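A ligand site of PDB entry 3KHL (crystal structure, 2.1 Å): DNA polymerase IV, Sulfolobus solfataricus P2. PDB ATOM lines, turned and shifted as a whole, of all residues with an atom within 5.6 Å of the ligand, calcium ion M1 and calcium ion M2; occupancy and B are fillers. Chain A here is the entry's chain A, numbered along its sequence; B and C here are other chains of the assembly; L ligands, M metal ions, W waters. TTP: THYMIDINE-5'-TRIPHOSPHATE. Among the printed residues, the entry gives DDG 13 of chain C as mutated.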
ATOM      1  N   PHE A   5      22.508 -15.952   3.070  1.00  0.00           N
ATOM      2  CA  PHE A   5      22.137 -17.055   3.948  1.00  0.00           C
ATOM      3  C   PHE A   5      23.109 -17.118   5.105  1.00  0.00           C
ATOM      4  O   PHE A   5      24.325 -17.005   4.893  1.00  0.00           O
ATOM      5  CB  PHE A   5      22.200 -18.355   3.140  1.00  0.00           C
ATOM      6  CG  PHE A   5      22.023 -19.600   3.953  1.00  0.00           C
ATOM      7  CD1 PHE A   5      20.756 -19.978   4.424  1.00  0.00           C
ATOM      8  CD2 PHE A   5      23.119 -20.437   4.225  1.00  0.00           C
ATOM      9  CE1 PHE A   5      20.599 -21.153   5.157  1.00  0.00           C
ATOM     10  CE2 PHE A   5      22.971 -21.589   4.963  1.00  0.00           C
ATOM     11  CZ  PHE A   5      21.726 -21.962   5.450  1.00  0.00           C
ATOM     12  N   ASP A   7      24.225 -19.411   8.621  1.00  0.00           N
ATOM     13  CA  ASP A   7      24.172 -20.738   9.234  1.00  0.00           C
ATOM     14  C   ASP A   7      25.217 -20.676  10.353  1.00  0.00           C
ATOM     15  O   ASP A   7      26.386 -20.397  10.073  1.00  0.00           O
ATOM     16  CB  ASP A   7      24.580 -21.768   8.159  1.00  0.00           C
ATOM     17  CG  ASP A   7      24.284 -23.219   8.548  1.00  0.00           C
ATOM     18  OD1 ASP A   7      24.153 -23.524   9.749  1.00  0.00           O
ATOM     19  OD2 ASP A   7      24.223 -24.075   7.618  1.00  0.00           O
ATOM     20  N   PHE A   8      24.801 -20.886  11.602  1.00  0.00           N
ATOM     21  CA  PHE A   8      25.667 -20.663  12.769  1.00  0.00           C
ATOM     22  C   PHE A   8      26.589 -21.863  12.917  1.00  0.00           C
ATOM     23  O   PHE A   8      26.151 -22.996  12.684  1.00  0.00           O
ATOM     24  CB  PHE A   8      24.850 -20.514  14.071  1.00  0.00           C
ATOM     25  CG  PHE A   8      23.675 -19.548  13.992  1.00  0.00           C
ATOM     26  CD1 PHE A   8      23.635 -18.519  13.052  1.00  0.00           C
ATOM     27  CD2 PHE A   8      22.628 -19.641  14.916  1.00  0.00           C
ATOM     28  CE1 PHE A   8      22.545 -17.650  13.000  1.00  0.00           C
ATOM     29  CE2 PHE A   8      21.519 -18.763  14.875  1.00  0.00           C
ATOM     30  CZ  PHE A   8      21.489 -17.765  13.920  1.00  0.00           C
ATOM     31  N   ASP A   9      27.837 -21.642  13.319  1.00  0.00           N
ATOM     32  CA  ASP A   9      28.828 -22.756  13.273  1.00  0.00           C
ATOM     33  C   ASP A   9      28.668 -23.696  14.444  1.00  0.00           C
ATOM     34  O   ASP A   9      28.527 -23.248  15.574  1.00  0.00           O
ATOM     35  CB  ASP A   9      30.313 -22.265  13.208  1.00  0.00           C
ATOM     36  CG  ASP A   9      30.604 -21.330  12.027  1.00  0.00           C
ATOM     37  OD1 ASP A   9      30.241 -21.581  10.866  1.00  0.00           O
ATOM     38  OD2 ASP A   9      31.321 -20.336  12.263  1.00  0.00           O
ATOM     39  N   TYR A  10      28.707 -25.003  14.169  1.00  0.00           N
ATOM     40  CA  TYR A  10      28.602 -26.090  15.175  1.00  0.00           C
ATOM     41  C   TYR A  10      27.711 -25.705  16.359  1.00  0.00           C
ATOM     42  O   TYR A  10      28.078 -25.820  17.532  1.00  0.00           O
ATOM     43  CB  TYR A  10      30.012 -26.660  15.569  1.00  0.00           C
ATOM     44  CG  TYR A  10      31.022 -25.673  16.173  1.00  0.00           C
ATOM     45  CD1 TYR A  10      31.282 -25.673  17.546  1.00  0.00           C
ATOM     46  CD2 TYR A  10      31.680 -24.745  15.377  1.00  0.00           C
ATOM     47  CE1 TYR A  10      32.210 -24.766  18.107  1.00  0.00           C
ATOM     48  CE2 TYR A  10      32.574 -23.835  15.922  1.00  0.00           C
ATOM     49  CZ  TYR A  10      32.832 -23.848  17.279  1.00  0.00           C
ATOM     50  OH  TYR A  10      33.717 -22.950  17.766  1.00  0.00           O
ATOM     51  N   PHE A  11      26.496 -25.276  16.014  1.00  0.00           N
ATOM     52  CA  PHE A  11      25.749 -24.374  16.901  1.00  0.00           C
ATOM     53  C   PHE A  11      25.656 -24.745  18.389  1.00  0.00           C
ATOM     54  O   PHE A  11      26.097 -23.970  19.233  1.00  0.00           O
ATOM     55  CB  PHE A  11      24.377 -24.017  16.328  1.00  0.00           C
ATOM     56  CG  PHE A  11      23.646 -22.962  17.099  1.00  0.00           C
ATOM     57  CD1 PHE A  11      24.288 -21.778  17.464  1.00  0.00           C
ATOM     58  CD2 PHE A  11      22.320 -23.153  17.459  1.00  0.00           C
ATOM     59  CE1 PHE A  11      23.600 -20.781  18.167  1.00  0.00           C
ATOM     60  CE2 PHE A  11      21.616 -22.165  18.177  1.00  0.00           C
ATOM     61  CZ  PHE A  11      22.237 -20.998  18.527  1.00  0.00           C
ATOM     62  N   TYR A  12      25.100 -25.921  18.722  1.00  0.00           N
ATOM     63  CA  TYR A  12      24.921 -26.230  20.160  1.00  0.00           C
ATOM     64  C   TYR A  12      26.209 -26.296  20.924  1.00  0.00           C
ATOM     65  O   TYR A  12      26.284 -25.839  22.069  1.00  0.00           O
ATOM     66  CB  TYR A  12      24.134 -27.513  20.408  1.00  0.00           C
ATOM     67  CG  TYR A  12      22.730 -27.556  19.850  1.00  0.00           C
ATOM     68  CD1 TYR A  12      22.098 -26.415  19.305  1.00  0.00           C
ATOM     69  CD2 TYR A  12      21.975 -28.743  19.928  1.00  0.00           C
ATOM     70  CE1 TYR A  12      20.791 -26.472  18.827  1.00  0.00           C
ATOM     71  CE2 TYR A  12      20.681 -28.819  19.453  1.00  0.00           C
ATOM     72  CZ  TYR A  12      20.090 -27.694  18.904  1.00  0.00           C
ATOM     73  OH  TYR A  12      18.831 -27.816  18.432  1.00  0.00           O
ATOM     74  N   ALA A  13      27.200 -26.917  20.280  1.00  0.00           N
ATOM     75  CA  ALA A  13      28.552 -27.050  20.800  1.00  0.00           C
ATOM     76  C   ALA A  13      29.218 -25.692  20.990  1.00  0.00           C
ATOM     77  O   ALA A  13      29.919 -25.460  21.986  1.00  0.00           O
ATOM     78  CB  ALA A  13      29.395 -27.923  19.839  1.00  0.00           C
ATOM     79  N   VAL A  43      24.053 -38.425  19.475  1.00  0.00           N
ATOM     80  CA  VAL A  43      24.730 -37.133  19.356  1.00  0.00           C
ATOM     81  C   VAL A  43      23.876 -36.132  18.587  1.00  0.00           C
ATOM     82  O   VAL A  43      23.338 -36.465  17.543  1.00  0.00           O
ATOM     83  CB  VAL A  43      26.152 -37.329  18.719  1.00  0.00           C
ATOM     84  CG1 VAL A  43      26.809 -36.017  18.331  1.00  0.00           C
ATOM     85  CG2 VAL A  43      27.044 -38.102  19.695  1.00  0.00           C
ATOM     86  N   ALA A  44      23.732 -34.921  19.136  1.00  0.00           N
ATOM     87  CA  ALA A  44      23.045 -33.803  18.501  1.00  0.00           C
ATOM     88  C   ALA A  44      24.012 -33.066  17.570  1.00  0.00           C
ATOM     89  O   ALA A  44      23.672 -32.724  16.439  1.00  0.00           O
ATOM     90  CB  ALA A  44      22.480 -32.833  19.582  1.00  0.00           C
ATOM     91  N   THR A  45      25.214 -32.811  18.076  1.00  0.00           N
ATOM     92  CA  THR A  45      26.298 -32.255  17.247  1.00  0.00           C
ATOM     93  C   THR A  45      27.605 -32.286  18.022  1.00  0.00           C
ATOM     94  O   THR A  45      27.629 -32.604  19.221  1.00  0.00           O
ATOM     95  CB  THR A  45      26.038 -30.808  16.774  1.00  0.00           C
ATOM     96  OG1 THR A  45      26.962 -30.474  15.737  1.00  0.00           O
ATOM     97  CG2 THR A  45      26.197 -29.795  17.925  1.00  0.00           C
ATOM     98  N   ALA A  46      28.685 -31.904  17.363  1.00  0.00           N
ATOM     99  CA  ALA A  46      29.964 -31.869  18.015  1.00  0.00           C
ATOM    100  C   ALA A  46      30.767 -30.759  17.376  1.00  0.00           C
ATOM    101  O   ALA A  46      30.472 -30.362  16.236  1.00  0.00           O
ATOM    102  CB  ALA A  46      30.685 -33.230  17.868  1.00  0.00           C
ATOM    103  N   TYR A  48      34.251 -29.015  15.754  1.00  0.00           N
ATOM    104  CA  TYR A  48      35.069 -29.514  14.669  1.00  0.00           C
ATOM    105  C   TYR A  48      36.210 -30.395  15.170  1.00  0.00           C
ATOM    106  O   TYR A  48      36.572 -31.357  14.492  1.00  0.00           O
ATOM    107  CB  TYR A  48      35.545 -28.372  13.766  1.00  0.00           C
ATOM    108  CG  TYR A  48      34.469 -27.963  12.772  1.00  0.00           C
ATOM    109  CD1 TYR A  48      33.369 -27.186  13.174  1.00  0.00           C
ATOM    110  CD2 TYR A  48      34.509 -28.402  11.429  1.00  0.00           C
ATOM    111  CE1 TYR A  48      32.347 -26.824  12.284  1.00  0.00           C
ATOM    112  CE2 TYR A  48      33.473 -28.035  10.520  1.00  0.00           C
ATOM    113  CZ  TYR A  48      32.412 -27.243  10.975  1.00  0.00           C
ATOM    114  OH  TYR A  48      31.416 -26.859  10.128  1.00  0.00           O
ATOM    115  N   ARG A  51      34.767 -33.746  15.425  1.00  0.00           N
ATOM    116  CA  ARG A  51      34.452 -34.288  14.099  1.00  0.00           C
ATOM    117  C   ARG A  51      35.630 -34.912  13.363  1.00  0.00           C
ATOM    118  O   ARG A  51      35.423 -35.861  12.589  1.00  0.00           O
ATOM    119  CB  ARG A  51      33.825 -33.254  13.192  1.00  0.00           C
ATOM    120  CG  ARG A  51      32.506 -32.748  13.717  1.00  0.00           C
ATOM    121  CD  ARG A  51      31.856 -31.833  12.735  1.00  0.00           C
ATOM    122  NE  ARG A  51      30.832 -31.062  13.437  1.00  0.00           N
ATOM    123  CZ  ARG A  51      29.989 -30.205  12.881  1.00  0.00           C
ATOM    124  NH1 ARG A  51      30.033 -29.973  11.564  1.00  0.00           N
ATOM    125  NH2 ARG A  51      29.122 -29.565  13.656  1.00  0.00           N
ATOM    126  N   ALA A  57      26.540 -35.539  14.296  1.00  0.00           N
ATOM    127  CA  ALA A  57      25.100 -35.614  14.536  1.00  0.00           C
ATOM    128  C   ALA A  57      24.540 -36.954  14.097  1.00  0.00           C
ATOM    129  O   ALA A  57      24.857 -37.421  13.025  1.00  0.00           O
ATOM    130  CB  ALA A  57      24.397 -34.471  13.826  1.00  0.00           C
ATOM    131  N   GLY A  58      23.744 -37.593  14.949  1.00  0.00           N
ATOM    132  CA  GLY A  58      23.067 -38.830  14.591  1.00  0.00           C
ATOM    133  C   GLY A  58      23.609 -40.106  15.189  1.00  0.00           C
ATOM    134  O   GLY A  58      22.862 -41.046  15.432  1.00  0.00           O
ATOM    135  N   MET A  76      22.250 -32.108  26.016  1.00  0.00           N
ATOM    136  CA  MET A  76      21.696 -31.051  25.186  1.00  0.00           C
ATOM    137  C   MET A  76      20.790 -30.155  26.039  1.00  0.00           C
ATOM    138  O   MET A  76      19.914 -30.656  26.750  1.00  0.00           O
ATOM    139  CB  MET A  76      20.901 -31.647  24.001  1.00  0.00           C
ATOM    140  CG  MET A  76      20.335 -30.605  23.041  1.00  0.00           C
ATOM    141  SD  MET A  76      19.085 -31.282  21.948  1.00  0.00           S
ATOM    142  CE  MET A  76      17.824 -31.910  23.059  1.00  0.00           C
ATOM    143  N   SER A 103      15.567 -22.724  10.357  1.00  0.00           N
ATOM    144  CA  SER A 103      15.849 -23.702  11.413  1.00  0.00           C
ATOM    145  C   SER A 103      16.329 -22.978  12.674  1.00  0.00           C
ATOM    146  O   SER A 103      16.403 -21.735  12.695  1.00  0.00           O
ATOM    147  CB  SER A 103      16.879 -24.735  10.950  1.00  0.00           C
ATOM    148  OG  SER A 103      18.199 -24.212  10.947  1.00  0.00           O
ATOM    149  N   ILE A 104      16.689 -23.734  13.712  1.00  0.00           N
ATOM    150  CA  ILE A 104      17.221 -23.126  14.916  1.00  0.00           C
ATOM    151  C   ILE A 104      18.481 -22.282  14.639  1.00  0.00           C
ATOM    152  O   ILE A 104      18.844 -21.422  15.437  1.00  0.00           O
ATOM    153  CB  ILE A 104      17.441 -24.158  16.054  1.00  0.00           C
ATOM    154  CG1 ILE A 104      17.575 -23.458  17.418  1.00  0.00           C
ATOM    155  CG2 ILE A 104      18.647 -25.085  15.769  1.00  0.00           C
ATOM    156  CD1 ILE A 104      17.292 -24.358  18.664  1.00  0.00           C
ATOM    157  N   ASP A 105      19.130 -22.505  13.494  1.00  0.00           N
ATOM    158  CA  ASP A 105      20.422 -21.836  13.248  1.00  0.00           C
ATOM    159  C   ASP A 105      20.692 -21.358  11.833  1.00  0.00           C
ATOM    160  O   ASP A 105      21.838 -21.186  11.434  1.00  0.00           O
ATOM    161  CB  ASP A 105      21.576 -22.712  13.767  1.00  0.00           C
ATOM    162  CG  ASP A 105      22.137 -23.665  12.724  1.00  0.00           C
ATOM    163  OD1 ASP A 105      21.376 -24.195  11.872  1.00  0.00           O
ATOM    164  OD2 ASP A 105      23.360 -23.860  12.729  1.00  0.00           O
ATOM    165  N   GLU A 106      19.624 -21.164  11.058  1.00  0.00           N
ATOM    166  CA  GLU A 106      19.691 -20.826   9.633  1.00  0.00           C
ATOM    167  C   GLU A 106      18.671 -19.759   9.332  1.00  0.00           C
ATOM    168  O   GLU A 106      17.530 -19.857   9.797  1.00  0.00           O
ATOM    169  CB  GLU A 106      19.271 -22.038   8.794  1.00  0.00           C
ATOM    170  CG  GLU A 106      20.372 -22.994   8.479  1.00  0.00           C
ATOM    171  CD  GLU A 106      19.943 -24.105   7.527  1.00  0.00           C
ATOM    172  OE1 GLU A 106      18.820 -24.059   6.988  1.00  0.00           O
ATOM    173  OE2 GLU A 106      20.767 -25.000   7.288  1.00  0.00           O
ATOM    174  N   LYS A 152      22.858 -21.246   0.040  1.00  0.00           N
ATOM    175  CA  LYS A 152      23.072 -22.286   1.026  1.00  0.00           C
ATOM    176  C   LYS A 152      24.279 -23.145   0.665  1.00  0.00           C
ATOM    177  O   LYS A 152      25.090 -23.499   1.525  1.00  0.00           O
ATOM    178  CB  LYS A 152      21.829 -23.166   1.214  1.00  0.00           C
ATOM    179  CG  LYS A 152      22.065 -24.303   2.217  1.00  0.00           C
ATOM    180  CD  LYS A 152      20.856 -25.219   2.293  1.00  0.00           C
ATOM    181  CE  LYS A 152      20.238 -25.194   3.671  1.00  0.00           C
ATOM    182  NZ  LYS A 152      21.116 -25.939   4.643  1.00  0.00           N
ATOM    183  N   LYS A 159      32.029 -23.142   5.280  1.00  0.00           N
ATOM    184  CA  LYS A 159      31.952 -23.607   6.692  1.00  0.00           C
ATOM    185  C   LYS A 159      33.301 -24.139   7.222  1.00  0.00           C
ATOM    186  O   LYS A 159      33.910 -24.907   6.536  1.00  0.00           O
ATOM    187  CB  LYS A 159      30.964 -24.801   6.779  1.00  0.00           C
ATOM    188  CG  LYS A 159      29.523 -24.437   7.063  1.00  0.00           C
ATOM    189  CD  LYS A 159      28.629 -25.650   7.315  1.00  0.00           C
ATOM    190  CE  LYS A 159      27.159 -25.232   7.190  1.00  0.00           C
ATOM    191  NZ  LYS A 159      26.131 -26.125   7.873  1.00  0.00           N
ATOM    192  N   PRO A 160      33.713 -23.804   8.471  1.00  0.00           N
ATOM    193  CA  PRO A 160      33.123 -22.899   9.498  1.00  0.00           C
ATOM    194  C   PRO A 160      33.698 -21.484   9.443  1.00  0.00           C
ATOM    195  O   PRO A 160      34.726 -21.257   8.814  1.00  0.00           O
ATOM    196  CB  PRO A 160      33.539 -23.563  10.828  1.00  0.00           C
ATOM    197  CG  PRO A 160      34.943 -24.131  10.519  1.00  0.00           C
ATOM    198  CD  PRO A 160      34.792 -24.639   9.046  1.00  0.00           C
ATOM    199  P    DA B   5      17.171 -43.148  19.102  1.00  0.00           P
ATOM    200  OP1  DA B   5      16.673 -44.034  20.183  1.00  0.00           O
ATOM    201  OP2  DA B   5      16.389 -42.984  17.862  1.00  0.00           O
ATOM    202  O5'  DA B   5      17.389 -41.701  19.740  1.00  0.00           O
ATOM    203  C5'  DA B   5      17.933 -41.552  21.058  1.00  0.00           C
ATOM    204  C4'  DA B   5      17.583 -40.157  21.520  1.00  0.00           C
ATOM    205  O4'  DA B   5      18.289 -39.169  20.736  1.00  0.00           O
ATOM    206  C3'  DA B   5      16.117 -39.792  21.385  1.00  0.00           C
ATOM    207  O3'  DA B   5      15.811 -38.928  22.436  1.00  0.00           O
ATOM    208  C2'  DA B   5      16.029 -39.047  20.046  1.00  0.00           C
ATOM    209  C1'  DA B   5      17.395 -38.387  19.976  1.00  0.00           C
ATOM    210  N9   DA B   5      17.991 -38.316  18.634  1.00  0.00           N
ATOM    211  C8   DA B   5      18.160 -39.315  17.716  1.00  0.00           C
ATOM    212  N7   DA B   5      18.749 -38.913  16.617  1.00  0.00           N
ATOM    213  C5   DA B   5      18.979 -37.566  16.818  1.00  0.00           C
ATOM    214  C6   DA B   5      19.579 -36.540  16.033  1.00  0.00           C
ATOM    215  N6   DA B   5      20.093 -36.694  14.802  1.00  0.00           N
ATOM    216  N1   DA B   5      19.627 -35.294  16.585  1.00  0.00           N
ATOM    217  C2   DA B   5      19.146 -35.076  17.808  1.00  0.00           C
ATOM    218  N3   DA B   5      18.573 -35.956  18.642  1.00  0.00           N
ATOM    219  C4   DA B   5      18.519 -37.187  18.067  1.00  0.00           C
ATOM    220  P    DC B   6      14.310 -38.706  22.935  1.00  0.00           P
ATOM    221  OP1  DC B   6      14.460 -38.369  24.372  1.00  0.00           O
ATOM    222  OP2  DC B   6      13.483 -39.860  22.522  1.00  0.00           O
ATOM    223  O5'  DC B   6      13.856 -37.423  22.094  1.00  0.00           O
ATOM    224  C5'  DC B   6      14.565 -36.224  22.330  1.00  0.00           C
ATOM    225  C4'  DC B   6      14.498 -35.330  21.123  1.00  0.00           C
ATOM    226  O4'  DC B   6      15.168 -35.944  20.013  1.00  0.00           O
ATOM    227  C3'  DC B   6      13.070 -35.075  20.642  1.00  0.00           C
ATOM    228  O3'  DC B   6      12.767 -33.758  21.041  1.00  0.00           O
ATOM    229  C2'  DC B   6      13.146 -35.245  19.124  1.00  0.00           C
ATOM    230  C1'  DC B   6      14.649 -35.260  18.912  1.00  0.00           C
ATOM    231  N1   DC B   6      15.127 -35.854  17.654  1.00  0.00           N
ATOM    232  C2   DC B   6      15.887 -35.002  16.816  1.00  0.00           C
ATOM    233  O2   DC B   6      16.110 -33.832  17.170  1.00  0.00           O
ATOM    234  N3   DC B   6      16.339 -35.481  15.642  1.00  0.00           N
ATOM    235  C4   DC B   6      16.072 -36.739  15.283  1.00  0.00           C
ATOM    236  N4   DC B   6      16.546 -37.124  14.106  1.00  0.00           N
ATOM    237  C5   DC B   6      15.306 -37.633  16.119  1.00  0.00           C
ATOM    238  C6   DC B   6      14.841 -37.147  17.284  1.00  0.00           C
ATOM    239  P   DDG C  13      20.779 -29.093   6.868  1.00  0.00           P
ATOM    240  OP1 DDG C  13      21.793 -28.102   7.273  1.00  0.00           O
ATOM    241  OP2 DDG C  13      21.122 -30.539   6.851  1.00  0.00           O
ATOM    242  O5' DDG C  13      19.449 -28.939   7.767  1.00  0.00           O
ATOM    243  C5' DDG C  13      18.917 -27.647   8.074  1.00  0.00           C
ATOM    244  C4' DDG C  13      18.525 -27.578   9.540  1.00  0.00           C
ATOM    245  O4' DDG C  13      17.631 -28.689   9.843  1.00  0.00           O
ATOM    246  C3' DDG C  13      19.675 -27.657  10.547  1.00  0.00           C
ATOM    247  C2' DDG C  13      19.106 -28.441  11.732  1.00  0.00           C
ATOM    248  C1' DDG C  13      17.921 -29.205  11.122  1.00  0.00           C
ATOM    249  N9  DDG C  13      18.078 -30.668  11.025  1.00  0.00           N
ATOM    250  C8  DDG C  13      18.460 -31.472   9.971  1.00  0.00           C
ATOM    251  N7  DDG C  13      18.460 -32.746  10.285  1.00  0.00           N
ATOM    252  C5  DDG C  13      18.031 -32.790  11.605  1.00  0.00           C
ATOM    253  C6  DDG C  13      17.814 -33.870  12.504  1.00  0.00           C
ATOM    254  O6  DDG C  13      17.952 -35.098  12.311  1.00  0.00           O
ATOM    255  N1  DDG C  13      17.379 -33.426  13.756  1.00  0.00           N
ATOM    256  C2  DDG C  13      17.179 -32.105  14.105  1.00  0.00           C
ATOM    257  N2  DDG C  13      16.768 -31.834  15.347  1.00  0.00           N
ATOM    258  N3  DDG C  13      17.386 -31.106  13.276  1.00  0.00           N
ATOM    259  C4  DDG C  13      17.794 -31.515  12.063  1.00  0.00           C
HETATM  260  PA  TTP L   1      23.585 -27.870  11.565  1.00  0.00           P
HETATM  261  O1A TTP L   1      23.732 -26.481  10.996  1.00  0.00           O
HETATM  262  O2A TTP L   1      23.328 -28.960  10.559  1.00  0.00           O
HETATM  263  O3A TTP L   1      24.916 -28.391  12.333  1.00  0.00           O
HETATM  264  PB  TTP L   1      25.963 -27.504  13.200  1.00  0.00           P
HETATM  265  O1B TTP L   1      25.640 -26.032  13.290  1.00  0.00           O
HETATM  266  O2B TTP L   1      26.067 -28.183  14.553  1.00  0.00           O
HETATM  267  O3B TTP L   1      27.361 -27.731  12.470  1.00  0.00           O
HETATM  268  PG  TTP L   1      27.897 -27.000  11.135  1.00  0.00           P
HETATM  269  O1G TTP L   1      29.100 -26.158  11.489  1.00  0.00           O
HETATM  270  O2G TTP L   1      28.420 -28.034  10.177  1.00  0.00           O
HETATM  271  O3G TTP L   1      26.908 -26.066  10.484  1.00  0.00           O
HETATM  272  O5' TTP L   1      22.451 -27.912  12.710  1.00  0.00           O
HETATM  273  C5' TTP L   1      22.346 -26.900  13.708  1.00  0.00           C
HETATM  274  C4' TTP L   1      21.996 -27.489  15.076  1.00  0.00           C
HETATM  275  O4' TTP L   1      20.832 -28.305  15.052  1.00  0.00           O
HETATM  276  C3' TTP L   1      23.096 -28.376  15.627  1.00  0.00           C
HETATM  277  O3' TTP L   1      24.097 -27.604  16.296  1.00  0.00           O
HETATM  278  C2' TTP L   1      22.343 -29.300  16.571  1.00  0.00           C
HETATM  279  C1' TTP L   1      20.958 -29.454  15.898  1.00  0.00           C
HETATM  280  N1  TTP L   1      20.984 -30.745  15.168  1.00  0.00           N
HETATM  281  C2  TTP L   1      20.549 -31.904  15.840  1.00  0.00           C
HETATM  282  O2  TTP L   1      20.126 -31.828  17.030  1.00  0.00           O
HETATM  283  N3  TTP L   1      20.561 -33.109  15.248  1.00  0.00           N
HETATM  284  C4  TTP L   1      21.009 -33.266  13.987  1.00  0.00           C
HETATM  285  O4  TTP L   1      21.004 -34.402  13.447  1.00  0.00           O
HETATM  286  C5  TTP L   1      21.499 -32.062  13.245  1.00  0.00           C
HETATM  287  C5M TTP L   1      21.987 -32.192  11.827  1.00  0.00           C
HETATM  288  C6  TTP L   1      21.454 -30.829  13.898  1.00  0.00           C
HETATM  289 CA    CA M   1      22.038 -25.409   9.801  1.00  0.00          CA
HETATM  290 CA    CA M   2      25.120 -24.686  11.505  1.00  0.00          CA
HETATM  291  O   HOH W   1      21.578 -35.591  11.240  1.00  0.00           O
HETATM  292  O   HOH W   2      22.798 -26.309   8.084  1.00  0.00           O
HETATM  293  O   HOH W   3      27.963 -23.177   9.603  1.00  0.00           O
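The side-chain hydroxyl (OH) of Tyr 48 lies within hydrogen-bond range of an oxygen (O1G) of the ligand.
The guanidinium group of Arg 51 lies within salt-bridge range of an oxygen (O2G) of the ligand (2.9 Å).
O1G of the ligand sits at hydrogen-bond distance from N of Tyr 10, at 2.9 Å.
An oxygen (O2B) of the ligand is in hydrogen-bond range of the side-chain hydroxyl (OG1) of Thr 45.
The backbone NH (N) of Tyr 12 is in hydrogen-bond range of an oxygen (O3') of the ligand (3.1 Å).
O2B of the ligand lies within hydrogen-bond range of N of Phe 11, 3.3 Å away.
O2G of the ligand lies within salt-bridge range of NZ of Lys 159 (3.8 Å).
N1 of DA 5 of chain B is in hydrogen-bond range of a nitrogen (N3) of the ligand (2.7 Å).
A nitrogen (N3) of the ligand lies close to the backbone carbonyl oxygen of Ala 44, at 3.4 Å.
The backbone carbonyl oxygen (O) of Ala 46 lies within hydrogen-bond range of the guanidinium group (NE) of Arg 51 (2.9 Å).
The backbone NH (N) of Asp 105 lies close to the side-chain hydroxyl (OG) of Ser 103.
NZ of Lys 159 is in salt-bridge range of OD2 of Asp 7 (2.8 Å).
The side-chain amino group of Lys 152 is in salt-bridge range of the side-chain carboxylate of Glu 106 (3.8 Å).
OP1 of DDG 13 of chain C is in salt-bridge range of the side-chain amino group of Lys 152 (3.5 Å).
NH2 of Arg 51 lies within hydrogen-bond range of OG1 of Thr 45, at 3.1 Å.
N of Glu 106 sits close to OG of Ser 103 (3.4 Å).
O6 of DDG 13 of chain C lies close to an oxygen (O4) of the ligand (3.3 Å).
Residues that only touch the ligand: Asp 9 (3.9 Å), Ala 57 (3.4 Å) and Ile 104 (3.96 Å).
Hydrophobic or aromatic side chains that line the ligand: Phe 11, Tyr 12, Ala 44, Tyr 48, Ala 57 and Ile 104.
Of the 27 residues printed, 16 come within 4 Å of the ligand.
The nearest printed residue that does not touch the ligand is Gly 58 (4.5 Å).
DDG 13 of chain C touches calcium ion M1 (C3' to CA, 3.3 Å).
Within 4 Å of calcium ion M1: Asp 7, Asp 105, Glu 106 and DDG 13 of chain C.
The nearest printed residue that does not touch calcium ion M1 is Ser 103 (4.2 Å).
Three residues have an atom within 4 Å of calcium ion M2: Asp 7, Phe 8 and Asp 105.
Calcium ion M1 is bound by water W2, an oxygen (O1A) of the ligand, the side-chain carboxylate (OD1) of Asp 105, the side-chain carboxylate (OD1) of Asp 7 and the side-chain carboxylate (OE2) of Glu 106.
Calcium ion M2 is bound by O1B of the ligand, OD2 of Asp 105, O of Phe 8, OD1 of Asp 7, O1A of the ligand and O3G of the ligand.
Calcium ion M2 has six donor atoms within binding distance.
Water W2 bridges OD2 of Asp 7 (2.7 Å) and NZ of Lys 159 (3.3 Å).
Water W3 bridges OD1 of Asp 9 (3.1 Å) and O of Asp 7 (3.2 Å).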
